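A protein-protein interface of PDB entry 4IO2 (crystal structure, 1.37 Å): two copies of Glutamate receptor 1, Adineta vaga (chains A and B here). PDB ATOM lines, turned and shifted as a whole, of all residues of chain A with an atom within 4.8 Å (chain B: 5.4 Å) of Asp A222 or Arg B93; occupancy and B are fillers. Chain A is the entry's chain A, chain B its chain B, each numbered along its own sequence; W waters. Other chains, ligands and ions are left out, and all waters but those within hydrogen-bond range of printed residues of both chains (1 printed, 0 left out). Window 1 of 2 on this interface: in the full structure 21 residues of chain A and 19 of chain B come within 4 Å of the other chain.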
ATOM      1  N   SER A  99      24.622 -14.999  21.909  1.00  0.00           N
ATOM      2  CA  SER A  99      23.289 -14.466  22.083  1.00  0.00           C
ATOM      3  C   SER A  99      22.275 -15.236  21.254  1.00  0.00           C
ATOM      4  O   SER A  99      22.610 -16.007  20.377  1.00  0.00           O
ATOM      5  CB  SER A  99      23.250 -12.995  21.650  1.00  0.00           C
ATOM      6  OG  SER A  99      23.259 -12.840  20.234  1.00  0.00           O
ATOM      7  N   ASN A 100      21.002 -14.979  21.509  1.00  0.00           N
ATOM      8  CA  ASN A 100      19.965 -15.436  20.609  1.00  0.00           C
ATOM      9  C   ASN A 100      20.310 -14.898  19.236  1.00  0.00           C
ATOM     10  O   ASN A 100      20.934 -13.837  19.082  1.00  0.00           O
ATOM     11  CB  ASN A 100      18.592 -14.947  21.086  1.00  0.00           C
ATOM     12  CG  ASN A 100      18.188 -15.591  22.372  1.00  0.00           C
ATOM     13  OD1 ASN A 100      18.059 -14.936  23.391  1.00  0.00           O
ATOM     14  ND2 ASN A 100      18.004 -16.904  22.342  1.00  0.00           N
ATOM     15  N   ALA A 218      23.825 -11.575  30.047  1.00  0.00           N
ATOM     16  CA  ALA A 218      23.252 -12.406  28.983  1.00  0.00           C
ATOM     17  C   ALA A 218      21.779 -12.138  28.746  1.00  0.00           C
ATOM     18  O   ALA A 218      21.331 -11.979  27.589  1.00  0.00           O
ATOM     19  CB  ALA A 218      23.499 -13.899  29.253  1.00  0.00           C
ATOM     20  N   LYS A 219      21.007 -12.087  29.812  1.00  0.00           N
ATOM     21  CA  LYS A 219      19.564 -11.909  29.680  1.00  0.00           C
ATOM     22  C   LYS A 219      19.244 -10.547  29.080  1.00  0.00           C
ATOM     23  O   LYS A 219      18.383 -10.421  28.200  1.00  0.00           O
ATOM     24  CB  LYS A 219      18.856 -12.089  31.028  1.00  0.00           C
ATOM     25  CG  LYS A 219      17.311 -11.963  30.975  1.00  0.00           C
ATOM     26  CD  LYS A 219      16.732 -12.028  32.349  1.00  0.00           C
ATOM     27  CE  LYS A 219      16.820 -10.679  33.001  1.00  0.00           C
ATOM     28  NZ  LYS A 219      15.949 -10.657  34.196  1.00  0.00           N
ATOM     29  N   ASP A 220      19.895  -9.496  29.546  1.00  0.00           N
ATOM     30  CA  ASP A 220      19.568  -8.151  29.027  1.00  0.00           C
ATOM     31  C   ASP A 220      19.788  -8.079  27.531  1.00  0.00           C
ATOM     32  O   ASP A 220      18.935  -7.582  26.788  1.00  0.00           O
ATOM     33  CB  ASP A 220      20.400  -7.072  29.803  1.00  0.00           C
ATOM     34  CG  ASP A 220      19.938  -5.614  29.579  1.00  0.00           C
ATOM     35  OD1 ASP A 220      18.740  -5.339  29.397  1.00  0.00           O
ATOM     36  OD2 ASP A 220      20.787  -4.683  29.685  1.00  0.00           O
ATOM     37  N   LEU A 221      20.901  -8.640  27.064  1.00  0.00           N
ATOM     38  CA  LEU A 221      21.191  -8.586  25.640  1.00  0.00           C
ATOM     39  C   LEU A 221      20.147  -9.425  24.890  1.00  0.00           C
ATOM     40  O   LEU A 221      19.608  -8.987  23.859  1.00  0.00           O
ATOM     41  CB  LEU A 221      22.611  -9.039  25.329  1.00  0.00           C
ATOM     42  CG  LEU A 221      22.990  -9.082  23.851  1.00  0.00           C
ATOM     43  CD1 LEU A 221      22.863  -7.687  23.211  1.00  0.00           C
ATOM     44  CD2 LEU A 221      24.365  -9.644  23.684  1.00  0.00           C
ATOM     45  N   ASP A 222      19.890 -10.641  25.352  1.00  0.00           N
ATOM     46  CA  ASP A 222      18.961 -11.540  24.653  1.00  0.00           C
ATOM     47  C   ASP A 222      17.552 -10.952  24.549  1.00  0.00           C
ATOM     48  O   ASP A 222      16.918 -11.006  23.496  1.00  0.00           O
ATOM     49  CB  ASP A 222      18.911 -12.930  25.338  1.00  0.00           C
ATOM     50  CG  ASP A 222      20.067 -13.842  24.952  1.00  0.00           C
ATOM     51  OD1 ASP A 222      20.891 -13.494  24.061  1.00  0.00           O
ATOM     52  OD2 ASP A 222      20.159 -14.917  25.601  1.00  0.00           O
ATOM     53  N   VAL A 223      17.019 -10.441  25.653  1.00  0.00           N
ATOM     54  CA  VAL A 223      15.686  -9.856  25.629  1.00  0.00           C
ATOM     55  C   VAL A 223      15.610  -8.716  24.600  1.00  0.00           C
ATOM     56  O   VAL A 223      14.618  -8.585  23.880  1.00  0.00           O
ATOM     57  CB  VAL A 223      15.289  -9.365  27.043  1.00  0.00           C
ATOM     58  CG1 VAL A 223      14.059  -8.459  27.028  1.00  0.00           C
ATOM     59  CG2 VAL A 223      15.066 -10.574  27.965  1.00  0.00           C
ATOM     60  N   ASN A 224      16.645  -7.890  24.541  1.00  0.00           N
ATOM     61  CA  ASN A 224      16.652  -6.811  23.611  1.00  0.00           C
ATOM     62  C   ASN A 224      16.795  -7.253  22.153  1.00  0.00           C
ATOM     63  O   ASN A 224      16.163  -6.667  21.271  1.00  0.00           O
ATOM     64  CB  ASN A 224      17.710  -5.784  24.007  1.00  0.00           C
ATOM     65  CG  ASN A 224      17.227  -4.859  25.061  1.00  0.00           C
ATOM     66  OD1 ASN A 224      16.560  -3.871  24.763  1.00  0.00           O
ATOM     67  ND2 ASN A 224      17.516  -5.177  26.315  1.00  0.00           N
ATOM     68  N   ILE A 225      17.633  -8.242  21.864  1.00  0.00           N
ATOM     69  CA  ILE A 225      17.676  -8.778  20.510  1.00  0.00           C
ATOM     70  C   ILE A 225      16.319  -9.313  20.083  1.00  0.00           C
ATOM     71  O   ILE A 225      15.866  -9.032  18.969  1.00  0.00           O
ATOM     72  CB  ILE A 225      18.749  -9.898  20.380  1.00  0.00           C
ATOM     73  CG1 ILE A 225      20.125  -9.315  20.552  1.00  0.00           C
ATOM     74  CG2 ILE A 225      18.598 -10.659  19.045  1.00  0.00           C
ATOM     75  CD1 ILE A 225      21.142 -10.397  20.787  1.00  0.00           C
ATOM     76  N   LEU A 226      15.661 -10.054  20.955  1.00  0.00           N
ATOM     77  CA  LEU A 226      14.360 -10.664  20.616  1.00  0.00           C
ATOM     78  C   LEU A 226      13.308  -9.574  20.407  1.00  0.00           C
ATOM     79  O   LEU A 226      12.458  -9.697  19.569  1.00  0.00           O
ATOM     80  CB  LEU A 226      13.971 -11.623  21.722  1.00  0.00           C
ATOM     81  CG  LEU A 226      14.812 -12.904  21.719  1.00  0.00           C
ATOM     82  CD1 LEU A 226      14.682 -13.656  23.055  1.00  0.00           C
ATOM     83  CD2 LEU A 226      14.409 -13.788  20.552  1.00  0.00           C
ATOM     84  N   THR B  89      10.817 -16.107  22.662  1.00  0.00           N
ATOM     85  CA  THR B  89      10.271 -14.753  22.673  1.00  0.00           C
ATOM     86  C   THR B  89      10.932 -13.919  23.745  1.00  0.00           C
ATOM     87  O   THR B  89      11.445 -14.448  24.713  1.00  0.00           O
ATOM     88  CB  THR B  89       8.737 -14.727  22.926  1.00  0.00           C
ATOM     89  OG1 THR B  89       8.489 -15.046  24.306  1.00  0.00           O
ATOM     90  CG2 THR B  89       7.959 -15.630  21.988  1.00  0.00           C
ATOM     91  N   SER B  90      10.869 -12.603  23.584  1.00  0.00           N
ATOM     92  CA  SER B  90      11.459 -11.682  24.550  1.00  0.00           C
ATOM     93  C   SER B  90      10.827 -11.816  25.925  1.00  0.00           C
ATOM     94  O   SER B  90      11.526 -11.825  26.928  1.00  0.00           O
ATOM     95  CB  SER B  90      11.351 -10.241  24.073  1.00  0.00           C
ATOM     96  OG  SER B  90       9.997  -9.794  23.921  1.00  0.00           O
ATOM     97  N   ALA B  91       9.513 -11.931  25.974  1.00  0.00           N
ATOM     98  CA  ALA B  91       8.835 -12.036  27.282  1.00  0.00           C
ATOM     99  C   ALA B  91       9.173 -13.344  27.965  1.00  0.00           C
ATOM    100  O   ALA B  91       9.294 -13.410  29.208  1.00  0.00           O
ATOM    101  CB  ALA B  91       7.321 -11.898  27.106  1.00  0.00           C
ATOM    102  N   ARG B  92       9.342 -14.424  27.206  1.00  0.00           N
ATOM    103  CA  ARG B  92       9.731 -15.691  27.859  1.00  0.00           C
ATOM    104  C   ARG B  92      11.186 -15.637  28.325  1.00  0.00           C
ATOM    105  O   ARG B  92      11.521 -16.142  29.397  1.00  0.00           O
ATOM    106  CB  ARG B  92       9.502 -16.860  26.926  1.00  0.00           C
ATOM    107  CG  ARG B  92       8.017 -17.158  26.674  1.00  0.00           C
ATOM    108  CD  ARG B  92       7.794 -18.033  25.480  1.00  0.00           C
ATOM    109  NE  ARG B  92       6.352 -18.190  25.227  1.00  0.00           N
ATOM    110  CZ  ARG B  92       5.853 -18.925  24.230  1.00  0.00           C
ATOM    111  NH1 ARG B  92       6.663 -19.558  23.400  1.00  0.00           N
ATOM    112  NH2 ARG B  92       4.534 -19.051  24.098  1.00  0.00           N
ATOM    113  N   ARG B  93      12.048 -15.005  27.542  1.00  0.00           N
ATOM    114  CA  ARG B  93      13.474 -14.916  27.845  1.00  0.00           C
ATOM    115  C   ARG B  93      13.734 -14.112  29.107  1.00  0.00           C
ATOM    116  O   ARG B  93      14.760 -14.294  29.752  1.00  0.00           O
ATOM    117  CB  ARG B  93      14.212 -14.318  26.643  1.00  0.00           C
ATOM    118  CG  ARG B  93      15.753 -14.210  26.824  1.00  0.00           C
ATOM    119  CD  ARG B  93      16.411 -15.572  26.981  1.00  0.00           C
ATOM    120  NE  ARG B  93      17.826 -15.488  27.311  1.00  0.00           N
ATOM    121  CZ  ARG B  93      18.315 -15.505  28.531  1.00  0.00           C
ATOM    122  NH1 ARG B  93      17.514 -15.472  29.576  1.00  0.00           N
ATOM    123  NH2 ARG B  93      19.624 -15.407  28.699  1.00  0.00           N
ATOM    124  N   GLU B  94      12.783 -13.274  29.505  1.00  0.00           N
ATOM    125  CA  GLU B  94      12.889 -12.557  30.763  1.00  0.00           C
ATOM    126  C   GLU B  94      12.928 -13.556  31.969  1.00  0.00           C
ATOM    127  O   GLU B  94      13.517 -13.253  33.038  1.00  0.00           O
ATOM    128  CB  GLU B  94      11.723 -11.499  30.853  1.00  0.00           C
ATOM    129  CG  GLU B  94      12.168 -10.024  30.506  1.00  0.00           C
ATOM    130  CD  GLU B  94      11.168  -9.089  29.736  1.00  0.00           C
ATOM    131  OE1 GLU B  94      10.270  -9.479  28.922  1.00  0.00           O
ATOM    132  OE2 GLU B  94      11.321  -7.883  29.914  1.00  0.00           O
ATOM    133  N   ILE B  95      12.285 -14.709  31.831  1.00  0.00           N
ATOM    134  CA  ILE B  95      12.103 -15.662  32.954  1.00  0.00           C
ATOM    135  C   ILE B  95      12.760 -17.049  32.845  1.00  0.00           C
ATOM    136  O   ILE B  95      12.896 -17.764  33.862  1.00  0.00           O
ATOM    137  CB  ILE B  95      10.604 -15.865  33.325  1.00  0.00           C
ATOM    138  CG1 ILE B  95       9.798 -16.390  32.144  1.00  0.00           C
ATOM    139  CG2 ILE B  95      10.003 -14.569  33.788  1.00  0.00           C
ATOM    140  CD1 ILE B  95       8.346 -16.860  32.547  1.00  0.00           C
ATOM    141  N   VAL B  96      13.135 -17.432  31.630  1.00  0.00           N
ATOM    142  CA  VAL B  96      13.840 -18.683  31.352  1.00  0.00           C
ATOM    143  C   VAL B  96      14.922 -18.398  30.325  1.00  0.00           C
ATOM    144  O   VAL B  96      14.905 -17.359  29.653  1.00  0.00           O
ATOM    145  CB  VAL B  96      12.893 -19.788  30.849  1.00  0.00           C
ATOM    146  CG1 VAL B  96      11.815 -20.108  31.890  1.00  0.00           C
ATOM    147  CG2 VAL B  96      12.294 -19.378  29.515  1.00  0.00           C
ATOM    148  N   ALA B  97      15.889 -19.305  30.245  1.00  0.00           N
ATOM    149  CA  ALA B  97      16.827 -19.293  29.126  1.00  0.00           C
ATOM    150  C   ALA B  97      16.372 -20.248  28.041  1.00  0.00           C
ATOM    151  O   ALA B  97      15.522 -21.107  28.266  1.00  0.00           O
ATOM    152  CB  ALA B  97      18.282 -19.609  29.608  1.00  0.00           C
ATOM    153  N   PHE B  98      16.924 -20.067  26.855  1.00  0.00           N
ATOM    154  CA  PHE B  98      16.703 -20.996  25.781  1.00  0.00           C
ATOM    155  C   PHE B  98      18.018 -21.527  25.275  1.00  0.00           C
ATOM    156  O   PHE B  98      18.993 -20.790  25.164  1.00  0.00           O
ATOM    157  CB  PHE B  98      15.968 -20.351  24.616  1.00  0.00           C
ATOM    158  CG  PHE B  98      14.529 -20.009  24.919  1.00  0.00           C
ATOM    159  CD1 PHE B  98      14.173 -18.801  25.508  1.00  0.00           C
ATOM    160  CD2 PHE B  98      13.532 -20.917  24.625  1.00  0.00           C
ATOM    161  CE1 PHE B  98      12.825 -18.510  25.754  1.00  0.00           C
ATOM    162  CE2 PHE B  98      12.243 -20.634  24.858  1.00  0.00           C
ATOM    163  CZ  PHE B  98      11.873 -19.428  25.407  1.00  0.00           C
ATOM    164  N   LYS B 213      17.247 -20.070  33.848  1.00  0.00           N
ATOM    165  CA  LYS B 213      18.260 -19.047  33.644  1.00  0.00           C
ATOM    166  C   LYS B 213      19.532 -19.430  34.398  1.00  0.00           C
ATOM    167  O   LYS B 213      19.484 -20.040  35.470  1.00  0.00           O
ATOM    168  CB  LYS B 213      17.762 -17.683  34.107  1.00  0.00           C
ATOM    169  CG  LYS B 213      16.643 -17.132  33.219  1.00  0.00           C
ATOM    170  CD  LYS B 213      16.295 -15.686  33.491  1.00  0.00           C
ATOM    171  CE  LYS B 213      15.781 -15.536  34.897  1.00  0.00           C
ATOM    172  NZ  LYS B 213      15.349 -14.128  35.108  1.00  0.00           N
HETATM  173  O   HOH W   1      17.751 -12.856  35.514  1.00  0.00           O
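The side-chain carboxylate of Asp A222 is in salt-bridge range of the guanidinium group of Arg B93, at 2.9 Å.
N of Asn A100 is in hydrogen-bond range of OD1 of Asp A222 (3.0 Å).
OG1 of Thr B89 is in hydrogen-bond range of N of Arg B92 (3.1 Å).
The guanidinium group (NH1) of Arg B93 sits at hydrogen-bond distance from the backbone carbonyl oxygen (O) of Val B96 (3.2 Å).
The backbone carbonyl oxygen of Glu B94 is in hydrogen-bond range of the side-chain amino group of Lys B213 (2.9 Å).
Asn A100 touches Arg B93 (OD1 to NE, 3.97 Å).
Arg B93 touches Ala A218 (NH2 to C, 3.9 Å).
Lys A219 touches Arg B93 (CA to NH2, 3.6 Å).
Lys B213 touches Lys A219.
Val A223 touches Ser B90.
Arg B93 touches Val A223.
Val A223 touches Glu B94 (CG2 to N, 3.9 Å).
Thr B89 touches Leu A226.
Leu A226 touches Ser B90.
Leu A226 touches Arg B93 (CD1 to CB, 3.7 Å).
Asp A222 touches one residue of chain B.
Of the printed residues of chain A, Arg B93 touches Asn A100 (3.97 Å), Ala A218 (3.9 Å), Lys A219 (3.6 Å), Asp A222 (2.9 Å), Val A223 (3.9 Å) and Leu A226 (3.7 Å).
Printed residues of chain A within 4 Å of Ser B90: Val A223 and Leu A226.
Of the printed residues of chain B, Lys A219 touches Arg B93 (3.6 Å), Glu B94 (3.5 Å) and Lys B213 (3.6 Å).
Of the printed residues of chain B, Ala A218 touches Arg B93.
Ser A99 touches none of the printed residues of chain B.
Ile A225 touches none of the printed residues of chain B.
The nearest printed residue of chain A that does not touch Lys B213 is Val A223 (7.6 Å).
Along chain B the printed residues that touch a printed residue of chain A span positions 89 to 213.
Among the printed residues, 12 pairs touch across the chains.
No position is printed for both chains.
Of the 12 pairs that touch across the chains among the printed residues, none has its exchanged pair printed and touching as well.
Water W1 bridges the side-chain amino group of Lys B213 and the side-chain amino group of Lys A219.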
